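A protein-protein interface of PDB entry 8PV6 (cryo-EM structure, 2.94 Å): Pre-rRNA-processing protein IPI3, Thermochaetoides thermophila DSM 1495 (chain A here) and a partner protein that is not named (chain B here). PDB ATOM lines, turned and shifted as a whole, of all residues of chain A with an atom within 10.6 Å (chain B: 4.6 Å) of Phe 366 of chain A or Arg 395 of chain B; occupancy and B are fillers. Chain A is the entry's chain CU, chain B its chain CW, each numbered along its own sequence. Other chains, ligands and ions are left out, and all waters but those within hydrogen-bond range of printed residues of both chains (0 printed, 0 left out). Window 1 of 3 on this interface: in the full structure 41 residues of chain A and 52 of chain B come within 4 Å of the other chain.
Of the printed residues of chain B, Pro 339 of chain A touches Arg 395 (3.2 Å) and Glu 397 (3.6 Å).
Printed residues of chain B within 4 Å of Thr 340 of chain A: Arg 395 (3.7 Å).
Of the printed residues of chain B, Phe 361 of chain A touches Asn 326 (3.7 Å) and Arg 395 (3.2 Å).
Printed residues of chain B within 4 Å of Glu 362 of chain A: Arg 395.
Phe 366 of chain A touches just these residues of chain B: Arg 394 and Arg 395.
Lys 368 of chain A touches none of the printed residues of chain B.
No residue of chain A comes within 4 Å of Asn 325 of chain B.
Printed residues of chain A within 4 Å of Asn 326 of chain B: Phe 361 (3.7 Å).
Ile 392 of chain B touches none of the printed residues of chain A.
Arg 394 of chain B touches just one residue of chain A: Phe 366.
Of the printed residues of chain A, Arg 395 of chain B touches Pro 339 (3.2 Å), Thr 340 (3.7 Å), Phe 361 (3.2 Å), Glu 362 (3.8 Å) and Phe 366 (3.2 Å).
The nearest residue of chain B that does not touch Phe 366 of chain A is Asn 325 of chain B (4.4 Å).
The nearest residue of chain A that does not touch Arg 395 of chain B is Met 364 of chain A (4.7 Å).
The nearest printed residue of chain B that does not touch Thr 340 of chain A is Leu 396 of chain B (4.9 Å).
The side-chain amide oxygen (OD1) of Asn 325 of chain B sits at hydrogen-bond distance from the guanidinium group (NH2) of Arg 394 of chain B, at 3.0 Å.
The backbone NH (N) of Glu 362 of chain A is in hydrogen-bond range of the backbone carbonyl oxygen (O) of Pro 339 of chain A, at 2.8 Å.
The guanidinium group (NH1) of Arg 395 of chain B sits at hydrogen-bond distance from the backbone carbonyl oxygen (O) of Phe 324 of chain B.
Among the printed residues, pairs that only touch across the chains: Pro 339 of chain A with Arg 395 of chain B, Pro 339 of chain A with Glu 397 of chain B, Thr 340 of chain A with Arg 395 of chain B, Phe 357 of chain A with Leu 396 of chain B, Phe 361 of chain A with Asn 326 of chain B, Phe 361 of chain A with Arg 395 of chain B, Glu 362 of chain A with Arg 395 of chain B, Phe 366 of chain A with Arg 394 of chain B and Phe 366 of chain A with Arg 395 of chain B.
Hydrophobic or aromatic side chains of chain B within 4 Å of the printed part of chain A: Leu 396.
Printed residues of chain A that touch a printed residue of chain B: Pro 339, Thr 340, Phe 357, Phe 361, Glu 362 and Phe 366.
Hydrophobic or aromatic side chains of chain A within 4 Å of the printed part of chain B: Pro 339, Phe 357, Phe 361 and Phe 366.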
ATOM      1  N   ASP A  97      28.147 -15.067  -6.467  1.00  0.00           N
ATOM      2  CA  ASP A  97      26.859 -15.151  -5.782  1.00  0.00           C
ATOM      3  C   ASP A  97      26.985 -15.728  -4.381  1.00  0.00           C
ATOM      4  O   ASP A  97      26.024 -16.293  -3.846  1.00  0.00           O
ATOM      5  CB  ASP A  97      25.887 -15.971  -6.621  1.00  0.00           C
ATOM      6  CG  ASP A  97      25.484 -15.264  -7.898  1.00  0.00           C
ATOM      7  OD1 ASP A  97      25.472 -14.016  -7.909  1.00  0.00           O
ATOM      8  OD2 ASP A  97      25.180 -15.956  -8.893  1.00  0.00           O
ATOM      9  N   CYS A 114      21.801 -17.338  -3.891  1.00  0.00           N
ATOM     10  CA  CYS A 114      20.811 -17.892  -4.809  1.00  0.00           C
ATOM     11  C   CYS A 114      20.198 -19.173  -4.261  1.00  0.00           C
ATOM     12  O   CYS A 114      19.024 -19.464  -4.515  1.00  0.00           O
ATOM     13  CB  CYS A 114      21.446 -18.143  -6.173  1.00  0.00           C
ATOM     14  SG  CYS A 114      22.268 -16.706  -6.890  1.00  0.00           S
ATOM     15  N   SER A 337      28.184  -8.937 -19.001  1.00  0.00           N
ATOM     16  CA  SER A 337      27.205  -9.935 -19.403  1.00  0.00           C
ATOM     17  C   SER A 337      27.295 -11.141 -18.480  1.00  0.00           C
ATOM     18  O   SER A 337      28.344 -11.786 -18.390  1.00  0.00           O
ATOM     19  CB  SER A 337      27.432 -10.359 -20.854  1.00  0.00           C
ATOM     20  OG  SER A 337      28.708 -10.956 -21.015  1.00  0.00           O
ATOM     21  N   LYS A 338      26.195 -11.438 -17.795  1.00  0.00           N
ATOM     22  CA  LYS A 338      26.119 -12.562 -16.882  1.00  0.00           C
ATOM     23  C   LYS A 338      24.889 -13.393 -17.220  1.00  0.00           C
ATOM     24  O   LYS A 338      23.786 -12.846 -17.341  1.00  0.00           O
ATOM     25  CB  LYS A 338      26.056 -12.079 -15.425  1.00  0.00           C
ATOM     26  CG  LYS A 338      26.054 -13.185 -14.386  1.00  0.00           C
ATOM     27  CD  LYS A 338      25.935 -12.611 -12.984  1.00  0.00           C
ATOM     28  CE  LYS A 338      25.637 -13.697 -11.967  1.00  0.00           C
ATOM     29  NZ  LYS A 338      25.524 -13.146 -10.590  1.00  0.00           N
ATOM     30  N   PRO A 339      25.049 -14.710 -17.395  1.00  0.00           N
ATOM     31  CA  PRO A 339      23.934 -15.542 -17.881  1.00  0.00           C
ATOM     32  C   PRO A 339      22.757 -15.657 -16.922  1.00  0.00           C
ATOM     33  O   PRO A 339      21.664 -16.024 -17.368  1.00  0.00           O
ATOM     34  CB  PRO A 339      24.591 -16.908 -18.110  1.00  0.00           C
ATOM     35  CG  PRO A 339      25.808 -16.891 -17.253  1.00  0.00           C
ATOM     36  CD  PRO A 339      26.292 -15.482 -17.252  1.00  0.00           C
ATOM     37  N   THR A 340      22.937 -15.366 -15.637  1.00  0.00           N
ATOM     38  CA  THR A 340      21.839 -15.375 -14.682  1.00  0.00           C
ATOM     39  C   THR A 340      21.798 -14.037 -13.960  1.00  0.00           C
ATOM     40  O   THR A 340      22.823 -13.379 -13.777  1.00  0.00           O
ATOM     41  CB  THR A 340      21.971 -16.511 -13.659  1.00  0.00           C
ATOM     42  OG1 THR A 340      23.235 -16.411 -12.992  1.00  0.00           O
ATOM     43  CG2 THR A 340      21.862 -17.863 -14.333  1.00  0.00           C
ATOM     44  N   LYS A 341      20.598 -13.636 -13.550  1.00  0.00           N
ATOM     45  CA  LYS A 341      20.410 -12.423 -12.766  1.00  0.00           C
ATOM     46  C   LYS A 341      19.778 -12.784 -11.432  1.00  0.00           C
ATOM     47  O   LYS A 341      18.756 -13.477 -11.391  1.00  0.00           O
ATOM     48  CB  LYS A 341      19.536 -11.401 -13.495  1.00  0.00           C
ATOM     49  CG  LYS A 341      19.817  -9.967 -13.072  1.00  0.00           C
ATOM     50  CD  LYS A 341      18.545  -9.147 -12.924  1.00  0.00           C
ATOM     51  CE  LYS A 341      17.740  -9.106 -14.207  1.00  0.00           C
ATOM     52  NZ  LYS A 341      16.516  -8.272 -14.058  1.00  0.00           N
ATOM     53  N   THR A 342      20.388 -12.313 -10.344  1.00  0.00           N
ATOM     54  CA  THR A 342      19.857 -12.535  -9.001  1.00  0.00           C
ATOM     55  C   THR A 342      18.901 -11.392  -8.678  1.00  0.00           C
ATOM     56  O   THR A 342      19.258 -10.393  -8.051  1.00  0.00           O
ATOM     57  CB  THR A 342      20.986 -12.636  -7.985  1.00  0.00           C
ATOM     58  OG1 THR A 342      21.991 -13.532  -8.475  1.00  0.00           O
ATOM     59  CG2 THR A 342      20.460 -13.160  -6.660  1.00  0.00           C
ATOM     60  N   PHE A 357      18.512 -23.870  -7.102  1.00  0.00           N
ATOM     61  CA  PHE A 357      19.156 -22.652  -7.570  1.00  0.00           C
ATOM     62  C   PHE A 357      18.086 -21.697  -8.079  1.00  0.00           C
ATOM     63  O   PHE A 357      17.326 -22.039  -8.990  1.00  0.00           O
ATOM     64  CB  PHE A 357      20.165 -22.971  -8.672  1.00  0.00           C
ATOM     65  CG  PHE A 357      20.941 -21.785  -9.149  1.00  0.00           C
ATOM     66  CD1 PHE A 357      21.951 -21.245  -8.374  1.00  0.00           C
ATOM     67  CD2 PHE A 357      20.671 -21.217 -10.380  1.00  0.00           C
ATOM     68  CE1 PHE A 357      22.671 -20.157  -8.817  1.00  0.00           C
ATOM     69  CE2 PHE A 357      21.385 -20.128 -10.826  1.00  0.00           C
ATOM     70  CZ  PHE A 357      22.386 -19.597 -10.043  1.00  0.00           C
ATOM     71  N   THR A 358      18.028 -20.504  -7.492  1.00  0.00           N
ATOM     72  CA  THR A 358      16.994 -19.524  -7.798  1.00  0.00           C
ATOM     73  C   THR A 358      17.623 -18.323  -8.488  1.00  0.00           C
ATOM     74  O   THR A 358      18.298 -17.515  -7.840  1.00  0.00           O
ATOM     75  CB  THR A 358      16.268 -19.077  -6.532  1.00  0.00           C
ATOM     76  OG1 THR A 358      17.165 -18.309  -5.723  1.00  0.00           O
ATOM     77  CG2 THR A 358      15.793 -20.281  -5.739  1.00  0.00           C
ATOM     78  N   ALA A 359      17.387 -18.198  -9.792  1.00  0.00           N
ATOM     79  CA  ALA A 359      17.849 -17.046 -10.553  1.00  0.00           C
ATOM     80  C   ALA A 359      17.007 -16.925 -11.811  1.00  0.00           C
ATOM     81  O   ALA A 359      16.309 -17.861 -12.205  1.00  0.00           O
ATOM     82  CB  ALA A 359      19.334 -17.159 -10.911  1.00  0.00           C
ATOM     83  N   GLN A 360      17.081 -15.754 -12.434  1.00  0.00           N
ATOM     84  CA  GLN A 360      16.430 -15.496 -13.710  1.00  0.00           C
ATOM     85  C   GLN A 360      17.430 -15.732 -14.830  1.00  0.00           C
ATOM     86  O   GLN A 360      18.538 -15.187 -14.803  1.00  0.00           O
ATOM     87  CB  GLN A 360      15.887 -14.068 -13.779  1.00  0.00           C
ATOM     88  CG  GLN A 360      15.503 -13.629 -15.182  1.00  0.00           C
ATOM     89  CD  GLN A 360      14.698 -12.351 -15.199  1.00  0.00           C
ATOM     90  OE1 GLN A 360      14.390 -11.783 -14.153  1.00  0.00           O
ATOM     91  NE2 GLN A 360      14.357 -11.885 -16.393  1.00  0.00           N
ATOM     92  N   PHE A 361      17.039 -16.541 -15.808  1.00  0.00           N
ATOM     93  CA  PHE A 361      17.928 -16.899 -16.905  1.00  0.00           C
ATOM     94  C   PHE A 361      17.929 -15.788 -17.948  1.00  0.00           C
ATOM     95  O   PHE A 361      16.893 -15.492 -18.552  1.00  0.00           O
ATOM     96  CB  PHE A 361      17.490 -18.225 -17.521  1.00  0.00           C
ATOM     97  CG  PHE A 361      17.860 -19.432 -16.699  1.00  0.00           C
ATOM     98  CD1 PHE A 361      18.713 -19.321 -15.613  1.00  0.00           C
ATOM     99  CD2 PHE A 361      17.350 -20.680 -17.016  1.00  0.00           C
ATOM    100  CE1 PHE A 361      19.050 -20.429 -14.861  1.00  0.00           C
ATOM    101  CE2 PHE A 361      17.683 -21.791 -16.267  1.00  0.00           C
ATOM    102  CZ  PHE A 361      18.534 -21.664 -15.189  1.00  0.00           C
ATOM    103  N   GLU A 362      19.089 -15.171 -18.154  1.00  0.00           N
ATOM    104  CA  GLU A 362      19.227 -14.082 -19.103  1.00  0.00           C
ATOM    105  C   GLU A 362      19.274 -14.618 -20.530  1.00  0.00           C
ATOM    106  O   GLU A 362      19.706 -15.748 -20.768  1.00  0.00           O
ATOM    107  CB  GLU A 362      20.486 -13.275 -18.793  1.00  0.00           C
ATOM    108  CG  GLU A 362      20.394 -12.465 -17.521  1.00  0.00           C
ATOM    109  CD  GLU A 362      19.446 -11.297 -17.656  1.00  0.00           C
ATOM    110  OE1 GLU A 362      19.375 -10.711 -18.758  1.00  0.00           O
ATOM    111  OE2 GLU A 362      18.764 -10.968 -16.668  1.00  0.00           O
ATOM    112  N   PRO A 363      18.833 -13.824 -21.512  1.00  0.00           N
ATOM    113  CA  PRO A 363      18.984 -14.243 -22.911  1.00  0.00           C
ATOM    114  C   PRO A 363      20.404 -14.040 -23.408  1.00  0.00           C
ATOM    115  O   PRO A 363      20.822 -12.905 -23.659  1.00  0.00           O
ATOM    116  CB  PRO A 363      17.990 -13.348 -23.667  1.00  0.00           C
ATOM    117  CG  PRO A 363      17.234 -12.583 -22.617  1.00  0.00           C
ATOM    118  CD  PRO A 363      18.086 -12.563 -21.400  1.00  0.00           C
ATOM    119  N   MET A 364      21.154 -15.130 -23.555  1.00  0.00           N
ATOM    120  CA  MET A 364      22.546 -15.070 -23.977  1.00  0.00           C
ATOM    121  C   MET A 364      22.764 -15.627 -25.377  1.00  0.00           C
ATOM    122  O   MET A 364      23.915 -15.704 -25.821  1.00  0.00           O
ATOM    123  CB  MET A 364      23.432 -15.814 -22.975  1.00  0.00           C
ATOM    124  CG  MET A 364      23.624 -15.091 -21.656  1.00  0.00           C
ATOM    125  SD  MET A 364      24.465 -13.511 -21.857  1.00  0.00           S
ATOM    126  CE  MET A 364      23.308 -12.404 -21.056  1.00  0.00           C
ATOM    127  N   SER A 365      21.684 -16.009 -26.072  1.00  0.00           N
ATOM    128  CA  SER A 365      21.729 -16.532 -27.443  1.00  0.00           C
ATOM    129  C   SER A 365      22.643 -17.752 -27.559  1.00  0.00           C
ATOM    130  O   SER A 365      23.463 -17.852 -28.473  1.00  0.00           O
ATOM    131  CB  SER A 365      22.140 -15.447 -28.443  1.00  0.00           C
ATOM    132  OG  SER A 365      23.545 -15.261 -28.442  1.00  0.00           O
ATOM    133  N   PHE A 366      22.505 -18.685 -26.614  1.00  0.00           N
ATOM    134  CA  PHE A 366      23.320 -19.895 -26.646  1.00  0.00           C
ATOM    135  C   PHE A 366      22.901 -20.815 -27.785  1.00  0.00           C
ATOM    136  O   PHE A 366      23.726 -21.559 -28.327  1.00  0.00           O
ATOM    137  CB  PHE A 366      23.231 -20.624 -25.305  1.00  0.00           C
ATOM    138  CG  PHE A 366      23.986 -19.949 -24.197  1.00  0.00           C
ATOM    139  CD1 PHE A 366      23.518 -19.995 -22.896  1.00  0.00           C
ATOM    140  CD2 PHE A 366      25.166 -19.274 -24.455  1.00  0.00           C
ATOM    141  CE1 PHE A 366      24.209 -19.377 -21.870  1.00  0.00           C
ATOM    142  CE2 PHE A 366      25.864 -18.652 -23.433  1.00  0.00           C
ATOM    143  CZ  PHE A 366      25.383 -18.705 -22.140  1.00  0.00           C
ATOM    144  N   THR A 367      21.628 -20.777 -28.165  1.00  0.00           N
ATOM    145  CA  THR A 367      21.098 -21.596 -29.245  1.00  0.00           C
ATOM    146  C   THR A 367      21.092 -20.788 -30.535  1.00  0.00           C
ATOM    147  O   THR A 367      20.614 -19.649 -30.555  1.00  0.00           O
ATOM    148  CB  THR A 367      19.685 -22.087 -28.922  1.00  0.00           C
ATOM    149  N   LYS A 368      21.625 -21.375 -31.603  1.00  0.00           N
ATOM    150  CA  LYS A 368      21.707 -20.727 -32.904  1.00  0.00           C
ATOM    151  C   LYS A 368      21.101 -21.627 -33.971  1.00  0.00           C
ATOM    152  O   LYS A 368      21.308 -22.843 -33.962  1.00  0.00           O
ATOM    153  CB  LYS A 368      23.159 -20.393 -33.265  1.00  0.00           C
ATOM    154  N   SER A 369      20.355 -21.019 -34.889  1.00  0.00           N
ATOM    155  CA  SER A 369      19.733 -21.726 -35.997  1.00  0.00           C
ATOM    156  C   SER A 369      20.088 -21.022 -37.298  1.00  0.00           C
ATOM    157  O   SER A 369      20.564 -19.884 -37.301  1.00  0.00           O
ATOM    158  CB  SER A 369      18.208 -21.806 -35.837  1.00  0.00           C
ATOM    159  N   ASP A 372      18.065 -17.919 -38.028  1.00  0.00           N
ATOM    160  CA  ASP A 372      18.496 -16.713 -37.329  1.00  0.00           C
ATOM    161  C   ASP A 372      19.421 -15.877 -38.201  1.00  0.00           C
ATOM    162  O   ASP A 372      19.465 -14.650 -38.068  1.00  0.00           O
ATOM    163  CB  ASP A 372      19.186 -17.079 -36.016  1.00  0.00           C
ATOM    164  CG  ASP A 372      18.247 -17.732 -35.026  1.00  0.00           C
ATOM    165  OD1 ASP A 372      17.030 -17.467 -35.097  1.00  0.00           O
ATOM    166  OD2 ASP A 372      18.725 -18.509 -34.175  1.00  0.00           O
ATOM    167  N   PHE B 324      18.208 -25.308 -19.878  1.00  0.00           N
ATOM    168  CA  PHE B 324      19.293 -24.403 -19.539  1.00  0.00           C
ATOM    169  C   PHE B 324      19.758 -23.576 -20.725  1.00  0.00           C
ATOM    170  O   PHE B 324      20.463 -22.583 -20.532  1.00  0.00           O
ATOM    171  CB  PHE B 324      20.473 -25.184 -18.962  1.00  0.00           C
ATOM    172  CG  PHE B 324      20.194 -25.775 -17.619  1.00  0.00           C
ATOM    173  CD1 PHE B 324      19.619 -27.029 -17.507  1.00  0.00           C
ATOM    174  CD2 PHE B 324      20.489 -25.069 -16.468  1.00  0.00           C
ATOM    175  CE1 PHE B 324      19.354 -27.569 -16.272  1.00  0.00           C
ATOM    176  CE2 PHE B 324      20.228 -25.606 -15.229  1.00  0.00           C
ATOM    177  CZ  PHE B 324      19.659 -26.857 -15.132  1.00  0.00           C
ATOM    178  N   ASN B 325      19.395 -23.967 -21.944  1.00  0.00           N
ATOM    179  CA  ASN B 325      19.698 -23.156 -23.112  1.00  0.00           C
ATOM    180  C   ASN B 325      18.652 -22.090 -23.411  1.00  0.00           C
ATOM    181  O   ASN B 325      18.897 -21.238 -24.270  1.00  0.00           O
ATOM    182  CB  ASN B 325      19.879 -24.049 -24.348  1.00  0.00           C
ATOM    183  CG  ASN B 325      21.207 -24.772 -24.350  1.00  0.00           C
ATOM    184  OD1 ASN B 325      22.099 -24.453 -23.568  1.00  0.00           O
ATOM    185  ND2 ASN B 325      21.346 -25.752 -25.232  1.00  0.00           N
ATOM    186  N   ASN B 326      17.497 -22.106 -22.732  1.00  0.00           N
ATOM    187  CA  ASN B 326      16.505 -21.069 -22.995  1.00  0.00           C
ATOM    188  C   ASN B 326      16.342 -20.132 -21.796  1.00  0.00           C
ATOM    189  O   ASN B 326      16.496 -20.553 -20.646  1.00  0.00           O
ATOM    190  CB  ASN B 326      15.145 -21.685 -23.342  1.00  0.00           C
ATOM    191  CG  ASN B 326      15.188 -22.496 -24.615  1.00  0.00           C
ATOM    192  OD1 ASN B 326      15.335 -21.948 -25.706  1.00  0.00           O
ATOM    193  ND2 ASN B 326      15.050 -23.807 -24.488  1.00  0.00           N
ATOM    194  N   ALA B 391      25.941 -27.837 -20.566  1.00  0.00           N
ATOM    195  CA  ALA B 391      24.961 -26.751 -20.574  1.00  0.00           C
ATOM    196  C   ALA B 391      24.764 -26.158 -19.184  1.00  0.00           C
ATOM    197  O   ALA B 391      24.642 -24.934 -19.037  1.00  0.00           O
ATOM    198  CB  ALA B 391      23.629 -27.245 -21.127  1.00  0.00           C
ATOM    199  N   ILE B 392      24.721 -27.010 -18.156  1.00  0.00           N
ATOM    200  CA  ILE B 392      24.587 -26.523 -16.783  1.00  0.00           C
ATOM    201  C   ILE B 392      25.797 -25.682 -16.390  1.00  0.00           C
ATOM    202  O   ILE B 392      25.655 -24.622 -15.769  1.00  0.00           O
ATOM    203  CB  ILE B 392      24.368 -27.702 -15.815  1.00  0.00           C
ATOM    204  CG1 ILE B 392      23.016 -28.362 -16.076  1.00  0.00           C
ATOM    205  CG2 ILE B 392      24.438 -27.244 -14.368  1.00  0.00           C
ATOM    206  CD1 ILE B 392      22.728 -29.539 -15.175  1.00  0.00           C
ATOM    207  N   ILE B 393      27.001 -26.128 -16.764  1.00  0.00           N
ATOM    208  CA  ILE B 393      28.211 -25.362 -16.477  1.00  0.00           C
ATOM    209  C   ILE B 393      28.184 -24.018 -17.197  1.00  0.00           C
ATOM    210  O   ILE B 393      28.510 -22.981 -16.605  1.00  0.00           O
ATOM    211  CB  ILE B 393      29.463 -26.181 -16.847  1.00  0.00           C
ATOM    212  CG1 ILE B 393      29.649 -27.348 -15.873  1.00  0.00           C
ATOM    213  CG2 ILE B 393      30.704 -25.302 -16.886  1.00  0.00           C
ATOM    214  CD1 ILE B 393      30.293 -26.970 -14.559  1.00  0.00           C
ATOM    215  N   ARG B 394      27.763 -24.004 -18.466  1.00  0.00           N
ATOM    216  CA  ARG B 394      27.731 -22.756 -19.223  1.00  0.00           C
ATOM    217  C   ARG B 394      26.713 -21.772 -18.655  1.00  0.00           C
ATOM    218  O   ARG B 394      26.971 -20.563 -18.617  1.00  0.00           O
ATOM    219  CB  ARG B 394      27.435 -23.036 -20.695  1.00  0.00           C
ATOM    220  CG  ARG B 394      27.681 -21.839 -21.602  1.00  0.00           C
ATOM    221  CD  ARG B 394      27.438 -22.179 -23.059  1.00  0.00           C
ATOM    222  NE  ARG B 394      26.380 -23.169 -23.218  1.00  0.00           N
ATOM    223  CZ  ARG B 394      25.911 -23.581 -24.387  1.00  0.00           C
ATOM    224  NH1 ARG B 394      26.383 -23.106 -25.527  1.00  0.00           N
ATOM    225  NH2 ARG B 394      24.941 -24.490 -24.412  1.00  0.00           N
ATOM    226  N   ARG B 395      25.552 -22.258 -18.216  1.00  0.00           N
ATOM    227  CA  ARG B 395      24.539 -21.350 -17.684  1.00  0.00           C
ATOM    228  C   ARG B 395      24.893 -20.860 -16.279  1.00  0.00           C
ATOM    229  O   ARG B 395      24.731 -19.676 -15.971  1.00  0.00           O
ATOM    230  CB  ARG B 395      23.164 -22.025 -17.712  1.00  0.00           C
ATOM    231  CG  ARG B 395      22.008 -21.239 -17.084  1.00  0.00           C
ATOM    232  CD  ARG B 395      21.913 -19.772 -17.522  1.00  0.00           C
ATOM    233  NE  ARG B 395      21.919 -19.555 -18.964  1.00  0.00           N
ATOM    234  CZ  ARG B 395      20.850 -19.641 -19.739  1.00  0.00           C
ATOM    235  NH1 ARG B 395      19.679 -20.018 -19.262  1.00  0.00           N
ATOM    236  NH2 ARG B 395      20.959 -19.342 -21.030  1.00  0.00           N
ATOM    237  N   LEU B 396      25.386 -21.745 -15.410  1.00  0.00           N
ATOM    238  CA  LEU B 396      25.590 -21.330 -14.024  1.00  0.00           C
ATOM    239  C   LEU B 396      26.926 -20.626 -13.817  1.00  0.00           C
ATOM    240  O   LEU B 396      27.010 -19.718 -12.981  1.00  0.00           O
ATOM    241  CB  LEU B 396      25.476 -22.530 -13.084  1.00  0.00           C
ATOM    242  CG  LEU B 396      24.185 -23.346 -13.126  1.00  0.00           C
ATOM    243  CD1 LEU B 396      24.142 -24.318 -11.963  1.00  0.00           C
ATOM    244  CD2 LEU B 396      22.968 -22.445 -13.115  1.00  0.00           C
ATOM    245  N   GLU B 397      27.966 -21.027 -14.558  1.00  0.00           N
ATOM    246  CA  GLU B 397      29.341 -20.528 -14.425  1.00  0.00           C
ATOM    247  C   GLU B 397      29.811 -20.796 -13.000  1.00  0.00           C
ATOM    248  O   GLU B 397      29.865 -21.973 -12.604  1.00  0.00           O
ATOM    249  CB  GLU B 397      29.422 -19.072 -14.894  1.00  0.00           C
ATOM    250  CG  GLU B 397      29.253 -18.896 -16.393  1.00  0.00           C
ATOM    251  CD  GLU B 397      29.421 -17.455 -16.833  1.00  0.00           C
ATOM    252  OE1 GLU B 397      29.571 -16.577 -15.957  1.00  0.00           O
ATOM    253  OE2 GLU B 397      29.404 -17.201 -18.055  1.00  0.00           O
